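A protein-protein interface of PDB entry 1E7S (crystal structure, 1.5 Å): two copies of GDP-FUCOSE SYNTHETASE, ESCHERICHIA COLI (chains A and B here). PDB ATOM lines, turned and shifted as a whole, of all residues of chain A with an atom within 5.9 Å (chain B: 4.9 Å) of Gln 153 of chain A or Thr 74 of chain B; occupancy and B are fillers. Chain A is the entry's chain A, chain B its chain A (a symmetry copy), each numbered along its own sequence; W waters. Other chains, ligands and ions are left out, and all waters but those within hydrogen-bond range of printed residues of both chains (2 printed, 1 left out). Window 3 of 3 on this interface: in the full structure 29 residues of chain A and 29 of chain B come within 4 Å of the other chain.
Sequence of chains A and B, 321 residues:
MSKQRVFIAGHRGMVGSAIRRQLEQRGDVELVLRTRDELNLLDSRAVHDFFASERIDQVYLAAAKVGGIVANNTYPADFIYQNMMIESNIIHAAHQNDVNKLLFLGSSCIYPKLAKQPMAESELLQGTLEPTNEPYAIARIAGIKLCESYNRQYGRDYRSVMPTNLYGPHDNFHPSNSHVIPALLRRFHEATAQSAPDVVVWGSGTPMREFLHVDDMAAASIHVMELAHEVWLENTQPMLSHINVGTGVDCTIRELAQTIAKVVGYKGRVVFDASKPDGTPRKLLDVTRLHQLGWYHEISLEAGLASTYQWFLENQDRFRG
Pro 76 of chain B touches Ser 149 of chain A (C to CB, 3.7 Å).
N of Ala 77 of chain B touches CB of Ser 149 of chain A, 3.5 Å away.
Ala 77 of chain B touches Tyr 150 of chain A.
Arg 152 of chain A touches Pro 76 of chain B.
Gln 153 of chain A touches Thr 74 of chain B.
Ala 77 of chain B touches Tyr 154 of chain A (CB to CE2, 3.9 Å).
Tyr 154 of chain A touches Asp 78 of chain B.
Along chain B the printed residues that touch a printed residue of chain A span positions 74 to 78.
Hydrophobic or aromatic side chains of chain A within 4 Å of the printed part of chain B: Tyr 150 and Tyr 154.
The side-chain hydroxyl of Tyr 154 of chain A is in hydrogen-bond range of the side-chain amide nitrogen of Gln 153 of chain A (3.2 Å).
OG1 of Thr 74 of chain B is in hydrogen-bond range of O of Val 70 of chain B (2.7 Å).
Of the printed residues of chain B, Gln 153 of chain A touches Thr 74, Tyr 75, Pro 76, Ala 77 and Asp 78.
Of the printed residues of chain B, Arg 152 of chain A touches Pro 76 (3.7 Å).
Of the printed residues of chain B, Tyr 150 of chain A touches Ala 77 (3.8 Å).
Printed residues of chain B within 4 Å of Ser 149 of chain A: Pro 76 (3.7 Å) and Ala 77 (3.5 Å).
Printed residues of chain A within 4 Å of Asp 78 of chain B: Gln 153 and Tyr 154.
The nearest printed residue of chain B that does not touch Arg 152 of chain A is Asn 73 of chain B (4.2 Å).
The side-chain amide oxygen (OE1) of Gln 153 of chain A sits close to the backbone carbonyl oxygen (O) of Tyr 75 of chain B (3.3 Å).
OE1 of Gln 153 of chain A sits at hydrogen-bond distance from N of Ala 77 of chain B (2.8 Å).
OD1 of Asp 78 of chain B sits at hydrogen-bond distance from NE2 of Gln 153 of chain A (2.9 Å).
OE1 of Gln 153 of chain A lies close to N of Pro 76 of chain B (3.3 Å).
No position is printed for both chains.
Of the 11 pairs that touch across the chains among the printed residues, none has its exchanged pair printed and touching as well.
Water W2 bridges the side-chain hydroxyl (OH) of Tyr 154 of chain A (2.7 Å) and the side-chain carboxylate (OD1) of Asp 78 of chain B (2.7 Å).
Water W1 lies within hydrogen-bond range of NH1 of Arg 152 of chain A and O of Asn 72 of chain B.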
ATOM      1  N   GLU A 148       0.782   1.474 -17.043  1.00  0.00           N
ATOM      2  CA  GLU A 148      -0.393   0.670 -16.728  1.00  0.00           C
ATOM      3  C   GLU A 148      -1.675   1.434 -17.044  1.00  0.00           C
ATOM      4  O   GLU A 148      -2.669   0.835 -17.491  1.00  0.00           O
ATOM      5  CB  GLU A 148      -0.379   0.289 -15.240  1.00  0.00           C
ATOM      6  CG  GLU A 148       0.756  -0.660 -14.905  1.00  0.00           C
ATOM      7  CD  GLU A 148       0.955  -0.995 -13.434  1.00  0.00           C
ATOM      8  OE1 GLU A 148       0.333  -0.380 -12.534  1.00  0.00           O
ATOM      9  OE2 GLU A 148       1.768  -1.924 -13.170  1.00  0.00           O
ATOM     10  N   SER A 149      -1.696   2.752 -16.849  1.00  0.00           N
ATOM     11  CA  SER A 149      -2.898   3.528 -17.091  1.00  0.00           C
ATOM     12  C   SER A 149      -3.189   3.648 -18.583  1.00  0.00           C
ATOM     13  O   SER A 149      -4.360   3.582 -18.982  1.00  0.00           O
ATOM     14  CB  SER A 149      -2.731   4.904 -16.425  1.00  0.00           C
ATOM     15  OG  SER A 149      -2.589   4.745 -15.022  1.00  0.00           O
ATOM     16  N   TYR A 150      -2.134   3.816 -19.419  1.00  0.00           N
ATOM     17  CA  TYR A 150      -2.364   3.781 -20.868  1.00  0.00           C
ATOM     18  C   TYR A 150      -2.787   2.393 -21.329  1.00  0.00           C
ATOM     19  O   TYR A 150      -3.648   2.248 -22.203  1.00  0.00           O
ATOM     20  CB  TYR A 150      -1.102   4.237 -21.618  1.00  0.00           C
ATOM     21  CG  TYR A 150      -0.971   5.748 -21.745  1.00  0.00           C
ATOM     22  CD1 TYR A 150      -0.528   6.552 -20.724  1.00  0.00           C
ATOM     23  CD2 TYR A 150      -1.427   6.382 -22.876  1.00  0.00           C
ATOM     24  CE1 TYR A 150      -0.445   7.923 -20.828  1.00  0.00           C
ATOM     25  CE2 TYR A 150      -1.371   7.752 -23.020  1.00  0.00           C
ATOM     26  CZ  TYR A 150      -0.857   8.526 -21.999  1.00  0.00           C
ATOM     27  OH  TYR A 150      -0.822   9.886 -22.204  1.00  0.00           O
ATOM     28  N   ASN A 151      -2.191   1.357 -20.716  1.00  0.00           N
ATOM     29  CA  ASN A 151      -2.652  -0.003 -21.064  1.00  0.00           C
ATOM     30  C   ASN A 151      -4.147  -0.200 -20.781  1.00  0.00           C
ATOM     31  O   ASN A 151      -4.880  -0.759 -21.632  1.00  0.00           O
ATOM     32  CB  ASN A 151      -1.868  -1.050 -20.285  1.00  0.00           C
ATOM     33  CG  ASN A 151      -0.400  -1.115 -20.660  1.00  0.00           C
ATOM     34  OD1 ASN A 151      -0.063  -0.660 -21.748  1.00  0.00           O
ATOM     35  ND2 ASN A 151       0.410  -1.734 -19.811  1.00  0.00           N
ATOM     36  N   ARG A 152      -4.578   0.239 -19.609  1.00  0.00           N
ATOM     37  CA  ARG A 152      -5.957   0.003 -19.175  1.00  0.00           C
ATOM     38  C   ARG A 152      -6.954   0.875 -19.917  1.00  0.00           C
ATOM     39  O   ARG A 152      -8.016   0.378 -20.332  1.00  0.00           O
ATOM     40  CB  ARG A 152      -6.067   0.157 -17.660  1.00  0.00           C
ATOM     41  CG  ARG A 152      -5.300  -0.887 -16.878  1.00  0.00           C
ATOM     42  CD  ARG A 152      -5.184  -0.505 -15.392  1.00  0.00           C
ATOM     43  NE  ARG A 152      -6.480  -0.493 -14.737  1.00  0.00           N
ATOM     44  CZ  ARG A 152      -6.986   0.449 -13.995  1.00  0.00           C
ATOM     45  NH1 ARG A 152      -6.324   1.582 -13.663  1.00  0.00           N
ATOM     46  NH2 ARG A 152      -8.227   0.260 -13.521  1.00  0.00           N
ATOM     47  N   GLN A 153      -6.603   2.171 -20.096  1.00  0.00           N
ATOM     48  CA  GLN A 153      -7.566   3.065 -20.736  1.00  0.00           C
ATOM     49  C   GLN A 153      -7.632   2.879 -22.260  1.00  0.00           C
ATOM     50  O   GLN A 153      -8.723   2.983 -22.850  1.00  0.00           O
ATOM     51  CB  GLN A 153      -7.178   4.521 -20.461  1.00  0.00           C
ATOM     52  CG  GLN A 153      -8.186   5.548 -21.017  1.00  0.00           C
ATOM     53  CD  GLN A 153      -7.897   6.949 -20.546  1.00  0.00           C
ATOM     54  OE1 GLN A 153      -7.266   7.195 -19.497  1.00  0.00           O
ATOM     55  NE2 GLN A 153      -8.422   7.933 -21.274  1.00  0.00           N
ATOM     56  N   TYR A 154      -6.478   2.646 -22.876  1.00  0.00           N
ATOM     57  CA  TYR A 154      -6.401   2.614 -24.327  1.00  0.00           C
ATOM     58  C   TYR A 154      -6.110   1.268 -24.989  1.00  0.00           C
ATOM     59  O   TYR A 154      -6.101   1.171 -26.237  1.00  0.00           O
ATOM     60  CB  TYR A 154      -5.362   3.636 -24.809  1.00  0.00           C
ATOM     61  CG  TYR A 154      -5.668   5.078 -24.429  1.00  0.00           C
ATOM     62  CD1 TYR A 154      -6.760   5.743 -25.026  1.00  0.00           C
ATOM     63  CD2 TYR A 154      -4.914   5.771 -23.508  1.00  0.00           C
ATOM     64  CE1 TYR A 154      -7.040   7.057 -24.758  1.00  0.00           C
ATOM     65  CE2 TYR A 154      -5.193   7.110 -23.227  1.00  0.00           C
ATOM     66  CZ  TYR A 154      -6.223   7.742 -23.879  1.00  0.00           C
ATOM     67  OH  TYR A 154      -6.491   9.064 -23.578  1.00  0.00           O
ATOM     68  N   GLY A 155      -5.820   0.251 -24.190  1.00  0.00           N
ATOM     69  CA  GLY A 155      -5.476  -1.073 -24.707  1.00  0.00           C
ATOM     70  C   GLY A 155      -4.065  -1.106 -25.319  1.00  0.00           C
ATOM     71  O   GLY A 155      -3.782  -1.946 -26.155  1.00  0.00           O
ATOM     72  N   VAL B  70     -16.247   6.375 -11.086  1.00  0.00           N
ATOM     73  CA  VAL B  70     -16.364   5.938 -12.472  1.00  0.00           C
ATOM     74  C   VAL B  70     -15.264   6.611 -13.290  1.00  0.00           C
ATOM     75  O   VAL B  70     -14.589   5.872 -14.043  1.00  0.00           O
ATOM     76  CB  VAL B  70     -17.732   6.209 -13.095  1.00  0.00           C
ATOM     77  CG1 VAL B  70     -17.733   5.903 -14.583  1.00  0.00           C
ATOM     78  CG2 VAL B  70     -18.849   5.426 -12.404  1.00  0.00           C
ATOM     79  N   ALA B  71     -15.082   7.929 -13.150  1.00  0.00           N
ATOM     80  CA  ALA B  71     -14.092   8.595 -13.991  1.00  0.00           C
ATOM     81  C   ALA B  71     -12.700   8.047 -13.695  1.00  0.00           C
ATOM     82  O   ALA B  71     -11.917   7.794 -14.635  1.00  0.00           O
ATOM     83  CB  ALA B  71     -14.130  10.078 -13.717  1.00  0.00           C
ATOM     84  N   ASN B  72     -12.334   7.889 -12.426  1.00  0.00           N
ATOM     85  CA  ASN B  72     -10.986   7.447 -12.088  1.00  0.00           C
ATOM     86  C   ASN B  72     -10.721   6.039 -12.652  1.00  0.00           C
ATOM     87  O   ASN B  72      -9.567   5.762 -12.991  1.00  0.00           O
ATOM     88  CB  ASN B  72     -10.722   7.523 -10.592  1.00  0.00           C
ATOM     89  CG  ASN B  72     -10.191   8.886 -10.176  1.00  0.00           C
ATOM     90  OD1 ASN B  72      -8.982   9.108 -10.184  1.00  0.00           O
ATOM     91  ND2 ASN B  72     -11.091   9.801  -9.840  1.00  0.00           N
ATOM     92  N   ASN B  73     -11.694   5.137 -12.644  1.00  0.00           N
ATOM     93  CA  ASN B  73     -11.465   3.813 -13.180  1.00  0.00           C
ATOM     94  C   ASN B  73     -11.512   3.782 -14.713  1.00  0.00           C
ATOM     95  O   ASN B  73     -11.011   2.820 -15.303  1.00  0.00           O
ATOM     96  CB  ASN B  73     -12.538   2.821 -12.674  1.00  0.00           C
ATOM     97  CG  ASN B  73     -12.281   2.385 -11.241  1.00  0.00           C
ATOM     98  OD1 ASN B  73     -11.276   1.709 -11.024  1.00  0.00           O
ATOM     99  ND2 ASN B  73     -13.094   2.701 -10.274  1.00  0.00           N
ATOM    100  N   THR B  74     -12.244   4.705 -15.323  1.00  0.00           N
ATOM    101  CA  THR B  74     -12.476   4.710 -16.758  1.00  0.00           C
ATOM    102  C   THR B  74     -11.385   5.417 -17.542  1.00  0.00           C
ATOM    103  O   THR B  74     -11.063   4.989 -18.654  1.00  0.00           O
ATOM    104  CB  THR B  74     -13.864   5.287 -17.053  1.00  0.00           C
ATOM    105  OG1 THR B  74     -14.879   4.505 -16.380  1.00  0.00           O
ATOM    106  CG2 THR B  74     -14.181   5.409 -18.528  1.00  0.00           C
ATOM    107  N   TYR B  75     -10.844   6.477 -16.955  1.00  0.00           N
ATOM    108  CA  TYR B  75      -9.832   7.283 -17.637  1.00  0.00           C
ATOM    109  C   TYR B  75      -8.572   7.429 -16.806  1.00  0.00           C
ATOM    110  O   TYR B  75      -8.056   8.535 -16.544  1.00  0.00           O
ATOM    111  CB  TYR B  75     -10.411   8.686 -17.907  1.00  0.00           C
ATOM    112  CG  TYR B  75     -11.751   8.717 -18.629  1.00  0.00           C
ATOM    113  CD1 TYR B  75     -11.791   8.526 -20.011  1.00  0.00           C
ATOM    114  CD2 TYR B  75     -12.961   8.900 -17.964  1.00  0.00           C
ATOM    115  CE1 TYR B  75     -12.977   8.533 -20.700  1.00  0.00           C
ATOM    116  CE2 TYR B  75     -14.153   8.899 -18.642  1.00  0.00           C
ATOM    117  CZ  TYR B  75     -14.167   8.698 -20.008  1.00  0.00           C
ATOM    118  OH  TYR B  75     -15.340   8.682 -20.740  1.00  0.00           O
ATOM    119  N   PRO B  76      -7.960   6.323 -16.412  1.00  0.00           N
ATOM    120  CA  PRO B  76      -6.812   6.393 -15.497  1.00  0.00           C
ATOM    121  C   PRO B  76      -5.674   7.186 -16.109  1.00  0.00           C
ATOM    122  O   PRO B  76      -4.965   7.883 -15.364  1.00  0.00           O
ATOM    123  CB  PRO B  76      -6.503   4.920 -15.194  1.00  0.00           C
ATOM    124  CG  PRO B  76      -7.030   4.159 -16.410  1.00  0.00           C
ATOM    125  CD  PRO B  76      -8.327   4.926 -16.717  1.00  0.00           C
ATOM    126  N   ALA B  77      -5.405   7.020 -17.411  1.00  0.00           N
ATOM    127  CA  ALA B  77      -4.274   7.756 -18.010  1.00  0.00           C
ATOM    128  C   ALA B  77      -4.507   9.255 -17.951  1.00  0.00           C
ATOM    129  O   ALA B  77      -3.566  10.001 -17.663  1.00  0.00           O
ATOM    130  CB  ALA B  77      -4.078   7.294 -19.466  1.00  0.00           C
ATOM    131  N   ASP B  78      -5.750   9.698 -18.138  1.00  0.00           N
ATOM    132  CA  ASP B  78      -6.020  11.158 -18.023  1.00  0.00           C
ATOM    133  C   ASP B  78      -5.632  11.643 -16.615  1.00  0.00           C
ATOM    134  O   ASP B  78      -5.012  12.700 -16.459  1.00  0.00           O
ATOM    135  CB  ASP B  78      -7.492  11.443 -18.199  1.00  0.00           C
ATOM    136  CG  ASP B  78      -8.115  11.271 -19.536  1.00  0.00           C
ATOM    137  OD1 ASP B  78      -7.602  10.627 -20.406  1.00  0.00           O
ATOM    138  OD2 ASP B  78      -9.342  11.639 -19.683  1.00  0.00           O
HETATM  139  O   HOH W   1      -7.936   3.070 -11.590  1.00  0.00           O
HETATM  140  O   HOH W   2      -5.131  10.129 -21.492  1.00  0.00           O
